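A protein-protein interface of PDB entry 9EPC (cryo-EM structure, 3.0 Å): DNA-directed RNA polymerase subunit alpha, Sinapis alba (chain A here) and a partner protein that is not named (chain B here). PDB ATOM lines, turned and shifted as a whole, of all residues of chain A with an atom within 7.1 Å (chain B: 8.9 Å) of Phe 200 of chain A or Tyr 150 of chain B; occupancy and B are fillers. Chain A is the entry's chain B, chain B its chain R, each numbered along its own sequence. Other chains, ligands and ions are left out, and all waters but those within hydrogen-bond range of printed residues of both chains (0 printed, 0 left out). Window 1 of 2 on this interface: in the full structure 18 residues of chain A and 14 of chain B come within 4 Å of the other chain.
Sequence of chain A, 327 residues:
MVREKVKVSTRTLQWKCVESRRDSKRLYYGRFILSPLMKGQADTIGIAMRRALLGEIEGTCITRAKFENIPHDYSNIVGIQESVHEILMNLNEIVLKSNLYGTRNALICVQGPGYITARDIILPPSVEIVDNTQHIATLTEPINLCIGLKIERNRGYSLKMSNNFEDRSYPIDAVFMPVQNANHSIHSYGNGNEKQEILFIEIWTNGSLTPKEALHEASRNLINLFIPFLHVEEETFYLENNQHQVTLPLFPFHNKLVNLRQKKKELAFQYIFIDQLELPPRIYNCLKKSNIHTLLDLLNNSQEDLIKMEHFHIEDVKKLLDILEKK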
ATOM      1  N   ARG A  11      -5.914  -0.601  -9.179  1.00  0.00           N
ATOM      2  CA  ARG A  11      -4.996  -1.290 -10.071  1.00  0.00           C
ATOM      3  C   ARG A  11      -4.390  -0.321 -11.078  1.00  0.00           C
ATOM      4  O   ARG A  11      -4.862   0.800 -11.272  1.00  0.00           O
ATOM      5  CB  ARG A  11      -5.707  -2.429 -10.806  1.00  0.00           C
ATOM      6  CG  ARG A  11      -5.873  -3.699 -10.000  1.00  0.00           C
ATOM      7  CD  ARG A  11      -6.348  -4.824 -10.899  1.00  0.00           C
ATOM      8  NE  ARG A  11      -5.464  -4.996 -12.047  1.00  0.00           N
ATOM      9  CZ  ARG A  11      -5.724  -5.778 -13.085  1.00  0.00           C
ATOM     10  NH1 ARG A  11      -6.847  -6.476 -13.160  1.00  0.00           N
ATOM     11  NH2 ARG A  11      -4.839  -5.860 -14.073  1.00  0.00           N
ATOM     12  N   VAL A  18      -3.343 -14.424 -22.085  1.00  0.00           N
ATOM     13  CA  VAL A  18      -4.186 -15.393 -21.393  1.00  0.00           C
ATOM     14  C   VAL A  18      -4.212 -16.715 -22.148  1.00  0.00           C
ATOM     15  O   VAL A  18      -4.309 -17.785 -21.539  1.00  0.00           O
ATOM     16  CB  VAL A  18      -5.608 -14.843 -21.189  1.00  0.00           C
ATOM     17  CG1 VAL A  18      -5.598 -13.756 -20.137  1.00  0.00           C
ATOM     18  CG2 VAL A  18      -6.163 -14.305 -22.489  1.00  0.00           C
ATOM     19  N   GLU A  19      -4.130 -16.657 -23.474  1.00  0.00           N
ATOM     20  CA  GLU A  19      -4.127 -17.853 -24.303  1.00  0.00           C
ATOM     21  C   GLU A  19      -3.000 -17.762 -25.315  1.00  0.00           C
ATOM     22  O   GLU A  19      -2.709 -16.684 -25.839  1.00  0.00           O
ATOM     23  CB  GLU A  19      -5.462 -18.042 -25.030  1.00  0.00           C
ATOM     24  CG  GLU A  19      -6.670 -18.090 -24.112  1.00  0.00           C
ATOM     25  CD  GLU A  19      -7.962 -18.358 -24.860  1.00  0.00           C
ATOM     26  OE1 GLU A  19      -7.922 -19.076 -25.881  1.00  0.00           O
ATOM     27  OE2 GLU A  19      -9.017 -17.847 -24.429  1.00  0.00           O
ATOM     28  N   ARG A  31      -4.189 -14.706 -27.257  1.00  0.00           N
ATOM     29  CA  ARG A  31      -5.218 -13.842 -26.701  1.00  0.00           C
ATOM     30  C   ARG A  31      -4.611 -13.021 -25.576  1.00  0.00           C
ATOM     31  O   ARG A  31      -3.928 -13.566 -24.706  1.00  0.00           O
ATOM     32  CB  ARG A  31      -6.404 -14.657 -26.188  1.00  0.00           C
ATOM     33  CG  ARG A  31      -7.665 -13.846 -25.998  1.00  0.00           C
ATOM     34  CD  ARG A  31      -8.702 -14.619 -25.214  1.00  0.00           C
ATOM     35  NE  ARG A  31      -9.965 -13.897 -25.140  1.00  0.00           N
ATOM     36  CZ  ARG A  31     -10.921 -14.154 -24.259  1.00  0.00           C
ATOM     37  NH1 ARG A  31     -10.778 -15.093 -23.338  1.00  0.00           N
ATOM     38  NH2 ARG A  31     -12.046 -13.446 -24.297  1.00  0.00           N
ATOM     39  N   PHE A  32      -4.857 -11.716 -25.597  1.00  0.00           N
ATOM     40  CA  PHE A  32      -4.243 -10.798 -24.650  1.00  0.00           C
ATOM     41  C   PHE A  32      -5.314  -9.958 -23.980  1.00  0.00           C
ATOM     42  O   PHE A  32      -6.313  -9.597 -24.606  1.00  0.00           O
ATOM     43  CB  PHE A  32      -3.225  -9.897 -25.345  1.00  0.00           C
ATOM     44  CG  PHE A  32      -2.181 -10.651 -26.108  1.00  0.00           C
ATOM     45  CD1 PHE A  32      -2.387 -11.001 -27.428  1.00  0.00           C
ATOM     46  CD2 PHE A  32      -0.996 -11.017 -25.503  1.00  0.00           C
ATOM     47  CE1 PHE A  32      -1.431 -11.698 -28.127  1.00  0.00           C
ATOM     48  CE2 PHE A  32      -0.038 -11.713 -26.200  1.00  0.00           C
ATOM     49  CZ  PHE A  32      -0.255 -12.054 -27.513  1.00  0.00           C
ATOM     50  N   ILE A  33      -5.099  -9.647 -22.707  1.00  0.00           N
ATOM     51  CA  ILE A  33      -6.039  -8.874 -21.907  1.00  0.00           C
ATOM     52  C   ILE A  33      -5.365  -7.579 -21.483  1.00  0.00           C
ATOM     53  O   ILE A  33      -4.185  -7.574 -21.117  1.00  0.00           O
ATOM     54  CB  ILE A  33      -6.526  -9.672 -20.682  1.00  0.00           C
ATOM     55  CG1 ILE A  33      -7.459  -8.820 -19.825  1.00  0.00           C
ATOM     56  CG2 ILE A  33      -5.355 -10.153 -19.850  1.00  0.00           C
ATOM     57  CD1 ILE A  33      -7.881  -9.487 -18.540  1.00  0.00           C
ATOM     58  N   LEU A  34      -6.105  -6.477 -21.560  1.00  0.00           N
ATOM     59  CA  LEU A  34      -5.642  -5.187 -21.073  1.00  0.00           C
ATOM     60  C   LEU A  34      -6.691  -4.624 -20.128  1.00  0.00           C
ATOM     61  O   LEU A  34      -7.861  -4.505 -20.501  1.00  0.00           O
ATOM     62  CB  LEU A  34      -5.388  -4.214 -22.224  1.00  0.00           C
ATOM     63  CG  LEU A  34      -4.832  -2.846 -21.834  1.00  0.00           C
ATOM     64  CD1 LEU A  34      -3.391  -2.970 -21.388  1.00  0.00           C
ATOM     65  CD2 LEU A  34      -4.954  -1.871 -22.986  1.00  0.00           C
ATOM     66  N   SER A  35      -6.274  -4.278 -18.916  1.00  0.00           N
ATOM     67  CA  SER A  35      -7.211  -3.814 -17.902  1.00  0.00           C
ATOM     68  C   SER A  35      -6.466  -3.141 -16.759  1.00  0.00           C
ATOM     69  O   SER A  35      -5.283  -3.427 -16.541  1.00  0.00           O
ATOM     70  CB  SER A  35      -8.041  -4.984 -17.375  1.00  0.00           C
ATOM     71  OG  SER A  35      -7.208  -5.959 -16.775  1.00  0.00           O
ATOM     72  N   LEU A  37      -9.567  -0.361 -17.917  1.00  0.00           N
ATOM     73  CA  LEU A  37      -9.703   0.730 -18.869  1.00  0.00           C
ATOM     74  C   LEU A  37     -10.957   1.528 -18.554  1.00  0.00           C
ATOM     75  O   LEU A  37     -11.991   0.960 -18.191  1.00  0.00           O
ATOM     76  CB  LEU A  37      -9.765   0.210 -20.304  1.00  0.00           C
ATOM     77  CG  LEU A  37      -8.452  -0.300 -20.889  1.00  0.00           C
ATOM     78  CD1 LEU A  37      -8.694  -0.965 -22.225  1.00  0.00           C
ATOM     79  CD2 LEU A  37      -7.477   0.846 -21.040  1.00  0.00           C
ATOM     80  N   ALA A  42     -11.501   1.292 -24.348  1.00  0.00           N
ATOM     81  CA  ALA A  42     -11.216  -0.047 -24.847  1.00  0.00           C
ATOM     82  C   ALA A  42     -11.568  -0.177 -26.322  1.00  0.00           C
ATOM     83  O   ALA A  42     -10.853  -0.838 -27.082  1.00  0.00           O
ATOM     84  CB  ALA A  42     -11.971  -1.084 -24.019  1.00  0.00           C
ATOM     85  N   GLY A  46      -8.870  -1.045 -29.208  1.00  0.00           N
ATOM     86  CA  GLY A  46      -9.097  -2.230 -30.018  1.00  0.00           C
ATOM     87  C   GLY A  46      -9.198  -1.923 -31.498  1.00  0.00           C
ATOM     88  O   GLY A  46      -8.703  -2.684 -32.333  1.00  0.00           O
ATOM     89  N   ASN A 183      -8.922  -9.636 -33.809  1.00  0.00           N
ATOM     90  CA  ASN A 183     -10.232  -9.270 -33.300  1.00  0.00           C
ATOM     91  C   ASN A 183     -10.085  -8.795 -31.865  1.00  0.00           C
ATOM     92  O   ASN A 183      -9.196  -9.241 -31.137  1.00  0.00           O
ATOM     93  CB  ASN A 183     -11.211 -10.444 -33.380  1.00  0.00           C
ATOM     94  CG  ASN A 183     -12.598 -10.077 -32.898  1.00  0.00           C
ATOM     95  OD1 ASN A 183     -12.966 -10.361 -31.760  1.00  0.00           O
ATOM     96  ND2 ASN A 183     -13.373  -9.433 -33.763  1.00  0.00           N
ATOM     97  N   HIS A 184     -10.966  -7.883 -31.464  1.00  0.00           N
ATOM     98  CA  HIS A 184     -10.952  -7.340 -30.116  1.00  0.00           C
ATOM     99  C   HIS A 184     -12.341  -7.441 -29.506  1.00  0.00           C
ATOM    100  O   HIS A 184     -13.353  -7.318 -30.199  1.00  0.00           O
ATOM    101  CB  HIS A 184     -10.475  -5.885 -30.098  1.00  0.00           C
ATOM    102  CG  HIS A 184     -11.512  -4.901 -30.529  1.00  0.00           C
ATOM    103  ND1 HIS A 184     -12.300  -4.210 -29.634  1.00  0.00           N
ATOM    104  CD2 HIS A 184     -11.892  -4.486 -31.761  1.00  0.00           C
ATOM    105  CE1 HIS A 184     -13.120  -3.413 -30.295  1.00  0.00           C
ATOM    106  NE2 HIS A 184     -12.893  -3.562 -31.587  1.00  0.00           N
ATOM    107  N   SER A 185     -12.376  -7.679 -28.199  1.00  0.00           N
ATOM    108  CA  SER A 185     -13.620  -7.798 -27.455  1.00  0.00           C
ATOM    109  C   SER A 185     -13.531  -6.961 -26.190  1.00  0.00           C
ATOM    110  O   SER A 185     -12.453  -6.783 -25.620  1.00  0.00           O
ATOM    111  CB  SER A 185     -13.923  -9.253 -27.099  1.00  0.00           C
ATOM    112  OG  SER A 185     -13.987 -10.056 -28.264  1.00  0.00           O
ATOM    113  N   ILE A 186     -14.677  -6.450 -25.754  1.00  0.00           N
ATOM    114  CA  ILE A 186     -14.760  -5.564 -24.601  1.00  0.00           C
ATOM    115  C   ILE A 186     -15.645  -6.217 -23.552  1.00  0.00           C
ATOM    116  O   ILE A 186     -16.772  -6.626 -23.851  1.00  0.00           O
ATOM    117  CB  ILE A 186     -15.317  -4.182 -24.984  1.00  0.00           C
ATOM    118  CG1 ILE A 186     -14.733  -3.713 -26.316  1.00  0.00           C
ATOM    119  CG2 ILE A 186     -15.033  -3.176 -23.887  1.00  0.00           C
ATOM    120  CD1 ILE A 186     -13.242  -3.541 -26.305  1.00  0.00           C
ATOM    121  N   HIS A 187     -15.136  -6.316 -22.329  1.00  0.00           N
ATOM    122  CA  HIS A 187     -15.916  -6.755 -21.181  1.00  0.00           C
ATOM    123  C   HIS A 187     -16.011  -5.595 -20.205  1.00  0.00           C
ATOM    124  O   HIS A 187     -14.986  -5.038 -19.800  1.00  0.00           O
ATOM    125  CB  HIS A 187     -15.289  -7.975 -20.507  1.00  0.00           C
ATOM    126  CG  HIS A 187     -15.399  -9.232 -21.308  1.00  0.00           C
ATOM    127  ND1 HIS A 187     -15.726  -9.236 -22.647  1.00  0.00           N
ATOM    128  CD2 HIS A 187     -15.234 -10.529 -20.957  1.00  0.00           C
ATOM    129  CE1 HIS A 187     -15.752 -10.482 -23.087  1.00  0.00           C
ATOM    130  NE2 HIS A 187     -15.457 -11.285 -22.082  1.00  0.00           N
ATOM    131  N   TYR A 189     -17.314  -4.188 -16.510  1.00  0.00           N
ATOM    132  CA  TYR A 189     -17.637  -4.609 -15.155  1.00  0.00           C
ATOM    133  C   TYR A 189     -18.036  -3.396 -14.332  1.00  0.00           C
ATOM    134  O   TYR A 189     -17.350  -2.368 -14.360  1.00  0.00           O
ATOM    135  CB  TYR A 189     -16.454  -5.328 -14.506  1.00  0.00           C
ATOM    136  CG  TYR A 189     -16.199  -6.702 -15.076  1.00  0.00           C
ATOM    137  CD1 TYR A 189     -15.475  -6.865 -16.246  1.00  0.00           C
ATOM    138  CD2 TYR A 189     -16.683  -7.835 -14.443  1.00  0.00           C
ATOM    139  CE1 TYR A 189     -15.241  -8.120 -16.769  1.00  0.00           C
ATOM    140  CE2 TYR A 189     -16.453  -9.092 -14.957  1.00  0.00           C
ATOM    141  CZ  TYR A 189     -15.732  -9.230 -16.120  1.00  0.00           C
ATOM    142  OH  TYR A 189     -15.501 -10.483 -16.636  1.00  0.00           O
ATOM    143  N   GLN A 196     -15.316   0.010 -15.072  1.00  0.00           N
ATOM    144  CA  GLN A 196     -14.048  -0.296 -15.711  1.00  0.00           C
ATOM    145  C   GLN A 196     -14.283  -1.253 -16.870  1.00  0.00           C
ATOM    146  O   GLN A 196     -15.195  -2.085 -16.836  1.00  0.00           O
ATOM    147  CB  GLN A 196     -13.051  -0.906 -14.720  1.00  0.00           C
ATOM    148  CG  GLN A 196     -13.333  -2.352 -14.352  1.00  0.00           C
ATOM    149  CD  GLN A 196     -12.213  -2.974 -13.545  1.00  0.00           C
ATOM    150  OE1 GLN A 196     -11.809  -4.107 -13.795  1.00  0.00           O
ATOM    151  NE2 GLN A 196     -11.706  -2.234 -12.566  1.00  0.00           N
ATOM    152  N   ILE A 198     -12.550  -4.028 -19.753  1.00  0.00           N
ATOM    153  CA  ILE A 198     -11.483  -4.985 -19.999  1.00  0.00           C
ATOM    154  C   ILE A 198     -11.419  -5.242 -21.495  1.00  0.00           C
ATOM    155  O   ILE A 198     -12.427  -5.607 -22.109  1.00  0.00           O
ATOM    156  CB  ILE A 198     -11.707  -6.295 -19.226  1.00  0.00           C
ATOM    157  CG1 ILE A 198     -11.585  -6.047 -17.723  1.00  0.00           C
ATOM    158  CG2 ILE A 198     -10.724  -7.352 -19.677  1.00  0.00           C
ATOM    159  CD1 ILE A 198     -11.763  -7.287 -16.888  1.00  0.00           C
ATOM    160  N   LEU A 199     -10.242  -5.050 -22.078  1.00  0.00           N
ATOM    161  CA  LEU A 199     -10.041  -5.220 -23.508  1.00  0.00           C
ATOM    162  C   LEU A 199      -9.335  -6.540 -23.773  1.00  0.00           C
ATOM    163  O   LEU A 199      -8.296  -6.825 -23.170  1.00  0.00           O
ATOM    164  CB  LEU A 199      -9.224  -4.064 -24.080  1.00  0.00           C
ATOM    165  CG  LEU A 199      -8.609  -4.292 -25.458  1.00  0.00           C
ATOM    166  CD1 LEU A 199      -9.683  -4.410 -26.518  1.00  0.00           C
ATOM    167  CD2 LEU A 199      -7.644  -3.177 -25.792  1.00  0.00           C
ATOM    168  N   PHE A 200      -9.900  -7.339 -24.670  1.00  0.00           N
ATOM    169  CA  PHE A 200      -9.301  -8.592 -25.108  1.00  0.00           C
ATOM    170  C   PHE A 200      -8.826  -8.423 -26.542  1.00  0.00           C
ATOM    171  O   PHE A 200      -9.607  -8.025 -27.411  1.00  0.00           O
ATOM    172  CB  PHE A 200     -10.294  -9.746 -25.012  1.00  0.00           C
ATOM    173  CG  PHE A 200     -10.580 -10.188 -23.612  1.00  0.00           C
ATOM    174  CD1 PHE A 200      -9.786 -11.139 -23.001  1.00  0.00           C
ATOM    175  CD2 PHE A 200     -11.644  -9.657 -22.909  1.00  0.00           C
ATOM    176  CE1 PHE A 200     -10.047 -11.549 -21.714  1.00  0.00           C
ATOM    177  CE2 PHE A 200     -11.908 -10.064 -21.623  1.00  0.00           C
ATOM    178  CZ  PHE A 200     -11.109 -11.011 -21.025  1.00  0.00           C
ATOM    179  N   ILE A 201      -7.558  -8.722 -26.787  1.00  0.00           N
ATOM    180  CA  ILE A 201      -6.992  -8.692 -28.129  1.00  0.00           C
ATOM    181  C   ILE A 201      -6.712 -10.120 -28.562  1.00  0.00           C
ATOM    182  O   ILE A 201      -6.079 -10.890 -27.831  1.00  0.00           O
ATOM    183  CB  ILE A 201      -5.712  -7.839 -28.185  1.00  0.00           C
ATOM    184  CG1 ILE A 201      -6.001  -6.414 -27.720  1.00  0.00           C
ATOM    185  CG2 ILE A 201      -5.159  -7.818 -29.593  1.00  0.00           C
ATOM    186  CD1 ILE A 201      -6.904  -5.650 -28.650  1.00  0.00           C
ATOM    187  N   GLU A 202      -7.187 -10.478 -29.750  1.00  0.00           N
ATOM    188  CA  GLU A 202      -7.056 -11.835 -30.268  1.00  0.00           C
ATOM    189  C   GLU A 202      -6.310 -11.759 -31.591  1.00  0.00           C
ATOM    190  O   GLU A 202      -6.782 -11.111 -32.529  1.00  0.00           O
ATOM    191  CB  GLU A 202      -8.429 -12.478 -30.445  1.00  0.00           C
ATOM    192  CG  GLU A 202      -8.482 -13.934 -30.069  1.00  0.00           C
ATOM    193  CD  GLU A 202      -9.897 -14.427 -29.876  1.00  0.00           C
ATOM    194  OE1 GLU A 202     -10.830 -13.602 -29.964  1.00  0.00           O
ATOM    195  OE2 GLU A 202     -10.079 -15.638 -29.630  1.00  0.00           O
ATOM    196  N   ARG B  73     -15.042 -20.421 -27.882  1.00  0.00           N
ATOM    197  CA  ARG B  73     -15.108 -19.775 -26.577  1.00  0.00           C
ATOM    198  C   ARG B  73     -16.475 -19.152 -26.341  1.00  0.00           C
ATOM    199  O   ARG B  73     -17.017 -19.231 -25.233  1.00  0.00           O
ATOM    200  CB  ARG B  73     -14.008 -18.724 -26.460  1.00  0.00           C
ATOM    201  CG  ARG B  73     -14.013 -17.973 -25.145  1.00  0.00           C
ATOM    202  CD  ARG B  73     -12.862 -16.991 -25.065  1.00  0.00           C
ATOM    203  NE  ARG B  73     -12.949 -15.955 -26.087  1.00  0.00           N
ATOM    204  CZ  ARG B  73     -12.243 -15.947 -27.210  1.00  0.00           C
ATOM    205  NH1 ARG B  73     -11.375 -16.906 -27.487  1.00  0.00           N
ATOM    206  NH2 ARG B  73     -12.413 -14.953 -28.075  1.00  0.00           N
ATOM    207  N   GLU B  77     -19.270 -20.195 -23.407  1.00  0.00           N
ATOM    208  CA  GLU B  77     -19.725 -19.153 -22.493  1.00  0.00           C
ATOM    209  C   GLU B  77     -21.229 -18.937 -22.601  1.00  0.00           C
ATOM    210  O   GLU B  77     -21.911 -18.762 -21.585  1.00  0.00           O
ATOM    211  CB  GLU B  77     -18.972 -17.853 -22.770  1.00  0.00           C
ATOM    212  CG  GLU B  77     -19.317 -16.722 -21.820  1.00  0.00           C
ATOM    213  CD  GLU B  77     -18.426 -15.511 -22.011  1.00  0.00           C
ATOM    214  OE1 GLU B  77     -17.552 -15.551 -22.904  1.00  0.00           O
ATOM    215  OE2 GLU B  77     -18.597 -14.522 -21.270  1.00  0.00           O
ATOM    216  N   GLU B 146     -19.646 -22.556 -15.190  1.00  0.00           N
ATOM    217  CA  GLU B 146     -18.432 -21.860 -15.584  1.00  0.00           C
ATOM    218  C   GLU B 146     -18.267 -20.609 -14.738  1.00  0.00           C
ATOM    219  O   GLU B 146     -19.245 -19.918 -14.438  1.00  0.00           O
ATOM    220  CB  GLU B 146     -18.458 -21.481 -17.069  1.00  0.00           C
ATOM    221  CG  GLU B 146     -17.154 -20.890 -17.577  1.00  0.00           C
ATOM    222  CD  GLU B 146     -17.330 -20.112 -18.864  1.00  0.00           C
ATOM    223  OE1 GLU B 146     -18.486 -19.804 -19.219  1.00  0.00           O
ATOM    224  OE2 GLU B 146     -16.312 -19.807 -19.518  1.00  0.00           O
ATOM    225  N   SER B 147     -17.027 -20.323 -14.357  1.00  0.00           N
ATOM    226  CA  SER B 147     -16.696 -19.124 -13.609  1.00  0.00           C
ATOM    227  C   SER B 147     -16.213 -18.038 -14.566  1.00  0.00           C
ATOM    228  O   SER B 147     -16.157 -18.222 -15.784  1.00  0.00           O
ATOM    229  CB  SER B 147     -15.640 -19.432 -12.545  1.00  0.00           C
ATOM    230  OG  SER B 147     -14.448 -19.917 -13.139  1.00  0.00           O
ATOM    231  N   ASP B 148     -15.855 -16.885 -14.001  1.00  0.00           N
ATOM    232  CA  ASP B 148     -15.330 -15.759 -14.768  1.00  0.00           C
ATOM    233  C   ASP B 148     -13.890 -15.518 -14.339  1.00  0.00           C
ATOM    234  O   ASP B 148     -13.639 -14.819 -13.346  1.00  0.00           O
ATOM    235  CB  ASP B 148     -16.181 -14.506 -14.554  1.00  0.00           C
ATOM    236  CG  ASP B 148     -15.821 -13.386 -15.508  1.00  0.00           C
ATOM    237  OD1 ASP B 148     -15.016 -13.626 -16.432  1.00  0.00           O
ATOM    238  OD2 ASP B 148     -16.341 -12.265 -15.335  1.00  0.00           O
ATOM    239  N   PRO B 149     -12.907 -16.073 -15.050  1.00  0.00           N
ATOM    240  CA  PRO B 149     -11.507 -15.905 -14.625  1.00  0.00           C
ATOM    241  C   PRO B 149     -11.017 -14.473 -14.686  1.00  0.00           C
ATOM    242  O   PRO B 149     -10.015 -14.149 -14.038  1.00  0.00           O
ATOM    243  CB  PRO B 149     -10.737 -16.803 -15.602  1.00  0.00           C
ATOM    244  CG  PRO B 149     -11.620 -16.897 -16.801  1.00  0.00           C
ATOM    245  CD  PRO B 149     -13.024 -16.871 -16.281  1.00  0.00           C
ATOM    246  N   TYR B 150     -11.687 -13.604 -15.440  1.00  0.00           N
ATOM    247  CA  TYR B 150     -11.264 -12.222 -15.605  1.00  0.00           C
ATOM    248  C   TYR B 150     -12.065 -11.256 -14.746  1.00  0.00           C
ATOM    249  O   TYR B 150     -11.973 -10.041 -14.946  1.00  0.00           O
ATOM    250  CB  TYR B 150     -11.357 -11.826 -17.077  1.00  0.00           C
ATOM    251  CG  TYR B 150     -10.827 -12.894 -17.999  1.00  0.00           C
ATOM    252  CD1 TYR B 150      -9.467 -13.162 -18.070  1.00  0.00           C
ATOM    253  CD2 TYR B 150     -11.684 -13.647 -18.787  1.00  0.00           C
ATOM    254  CE1 TYR B 150      -8.977 -14.142 -18.905  1.00  0.00           C
ATOM    255  CE2 TYR B 150     -11.202 -14.630 -19.627  1.00  0.00           C
ATOM    256  CZ  TYR B 150      -9.847 -14.873 -19.682  1.00  0.00           C
ATOM    257  OH  TYR B 150      -9.361 -15.851 -20.517  1.00  0.00           O
ATOM    258  N   LYS B 151     -12.839 -11.763 -13.800  1.00  0.00           N
ATOM    259  CA  LYS B 151     -13.610 -10.900 -12.917  1.00  0.00           C
ATOM    260  C   LYS B 151     -12.660 -10.144 -11.998  1.00  0.00           C
ATOM    261  O   LYS B 151     -11.894 -10.778 -11.260  1.00  0.00           O
ATOM    262  CB  LYS B 151     -14.601 -11.737 -12.116  1.00  0.00           C
ATOM    263  CG  LYS B 151     -15.482 -10.958 -11.161  1.00  0.00           C
ATOM    264  CD  LYS B 151     -16.649 -11.820 -10.706  1.00  0.00           C
ATOM    265  CE  LYS B 151     -17.261 -11.308  -9.417  1.00  0.00           C
ATOM    266  NZ  LYS B 151     -16.314 -11.436  -8.278  1.00  0.00           N
ATOM    267  N   PRO B 152     -12.661  -8.813 -12.015  1.00  0.00           N
ATOM    268  CA  PRO B 152     -11.666  -8.061 -11.238  1.00  0.00           C
ATOM    269  C   PRO B 152     -11.852  -8.162  -9.732  1.00  0.00           C
ATOM    270  O   PRO B 152     -10.905  -8.482  -9.007  1.00  0.00           O
ATOM    271  CB  PRO B 152     -11.860  -6.621 -11.728  1.00  0.00           C
ATOM    272  CG  PRO B 152     -13.260  -6.577 -12.224  1.00  0.00           C
ATOM    273  CD  PRO B 152     -13.541  -7.930 -12.798  1.00  0.00           C
ATOM    274  N   GLY B 153     -13.062  -7.897  -9.248  1.00  0.00           N
ATOM    275  CA  GLY B 153     -13.311  -7.856  -7.828  1.00  0.00           C
ATOM    276  C   GLY B 153     -14.628  -8.495  -7.439  1.00  0.00           C
ATOM    277  O   GLY B 153     -15.490  -8.761  -8.282  1.00  0.00           O
ATOM    278  N   TYR B 156     -17.652  -6.450  -8.491  1.00  0.00           N
ATOM    279  CA  TYR B 156     -17.777  -6.179  -9.918  1.00  0.00           C
ATOM    280  C   TYR B 156     -18.528  -7.328 -10.576  1.00  0.00           C
ATOM    281  O   TYR B 156     -18.040  -8.462 -10.607  1.00  0.00           O
ATOM    282  CB  TYR B 156     -16.401  -5.991 -10.552  1.00  0.00           C
ATOM    283  CG  TYR B 156     -15.707  -4.715 -10.147  1.00  0.00           C
ATOM    284  CD1 TYR B 156     -14.931  -4.658  -8.999  1.00  0.00           C
ATOM    285  CD2 TYR B 156     -15.824  -3.565 -10.915  1.00  0.00           C
ATOM    286  CE1 TYR B 156     -14.293  -3.493  -8.626  1.00  0.00           C
ATOM    287  CE2 TYR B 156     -15.191  -2.396 -10.551  1.00  0.00           C
ATOM    288  CZ  TYR B 156     -14.427  -2.365  -9.405  1.00  0.00           C
ATOM    289  OH  TYR B 156     -13.794  -1.200  -9.039  1.00  0.00           O
ATOM    290  N   LYS B 158     -20.355  -8.619 -14.191  1.00  0.00           N
ATOM    291  CA  LYS B 158     -20.138  -8.386 -15.615  1.00  0.00           C
ATOM    292  C   LYS B 158     -21.370  -7.740 -16.234  1.00  0.00           C
ATOM    293  O   LYS B 158     -22.401  -8.394 -16.414  1.00  0.00           O
ATOM    294  CB  LYS B 158     -19.806  -9.701 -16.313  1.00  0.00           C
ATOM    295  CG  LYS B 158     -19.435  -9.551 -17.777  1.00  0.00           C
ATOM    296  CD  LYS B 158     -19.198 -10.903 -18.426  1.00  0.00           C
ATOM    297  CE  LYS B 158     -18.680 -10.755 -19.845  1.00  0.00           C
ATOM    298  NZ  LYS B 158     -19.598  -9.951 -20.695  1.00  0.00           N
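OD1 of Asp 148 of chain B lies close to OH of Tyr 189 of chain A.
OE2 of Glu 19 of chain A is in salt-bridge range of NH1 of Arg 73 of chain B (3.97 Å).
NH2 of Arg 31 of chain A lies close to NE of Arg 73 of chain B.
The guanidinium group (NH1) of Arg 31 of chain A is in hydrogen-bond range of the side-chain hydroxyl (OH) of Tyr 150 of chain B (3.2 Å).
The side-chain carboxylate (OE2) of Glu 202 of chain A lies within salt-bridge range of the guanidinium group (NH1) of Arg 73 of chain B.
The backbone NH (N) of Val 18 of chain A is in hydrogen-bond range of the backbone carbonyl oxygen (O) of Arg 31 of chain A, 2.8 Å away.
N of Phe 200 of chain A sits at hydrogen-bond distance from O of Ser 185 of chain A, 2.8 Å away.
The backbone carbonyl oxygen (O) of Asn 183 of chain A sits at hydrogen-bond distance from the backbone NH (N) of Glu 202 of chain A (2.7 Å).
OE2 of Glu 19 of chain A lies within salt-bridge range of NH1 of Arg 31 of chain A (3.4 Å).
The side-chain amino group (NZ) of Lys 151 of chain B sits at hydrogen-bond distance from the backbone carbonyl oxygen (O) of Gly 153 of chain B, at 2.8 Å.
O of Gln 196 of chain A is in hydrogen-bond range of N of Tyr 189 of chain A, at 3.0 Å.
Among the printed residues, merely in contact across the chains: Val 18 of chain A with Tyr 150 of chain B, His 187 of chain A with Lys 158 of chain B, Tyr 189 of chain A with Tyr 150 of chain B, Tyr 189 of chain A with Lys 151 of chain B, Tyr 189 of chain A with Pro 152 of chain B, Tyr 189 of chain A with Tyr 156 of chain B, Tyr 189 of chain A with Lys 158 of chain B, Gln 196 of chain A with Pro 152 of chain B, Ile 198 of chain A with Tyr 150 of chain B and Phe 200 of chain A with Tyr 150 of chain B.
Of the printed residues of chain B, Val 18 of chain A touches Tyr 150.
Printed residues of chain B within 4 Å of Gln 196 of chain A: Pro 152.
Of the printed residues of chain B, Ile 198 of chain A touches Tyr 150 (3.4 Å).
Phe 200 of chain A touches just one residue of chain B: Tyr 150.
No residue of chain B comes within 4 Å of Ile 201 of chain A.
Of chain A, only Val 18, Arg 31, Tyr 189, Ile 198 and Phe 200 come within 4 Å of Tyr 150 of chain B.
Of the 12 printed residues of chain B, 7 touch a printed residue of chain A.
Hydrophobic or aromatic side chains of chain B that line the printed part of chain A: Tyr 150, Pro 152 and Tyr 156.
Of the 23 printed residues of chain A, 9 touch a printed residue of chain B.
Hydrophobic or aromatic side chains of chain A that line the printed part of chain B: Val 18, His 187, Tyr 189, Ile 198 and Phe 200.
Among the printed residues, 15 pairs touch across the chains.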
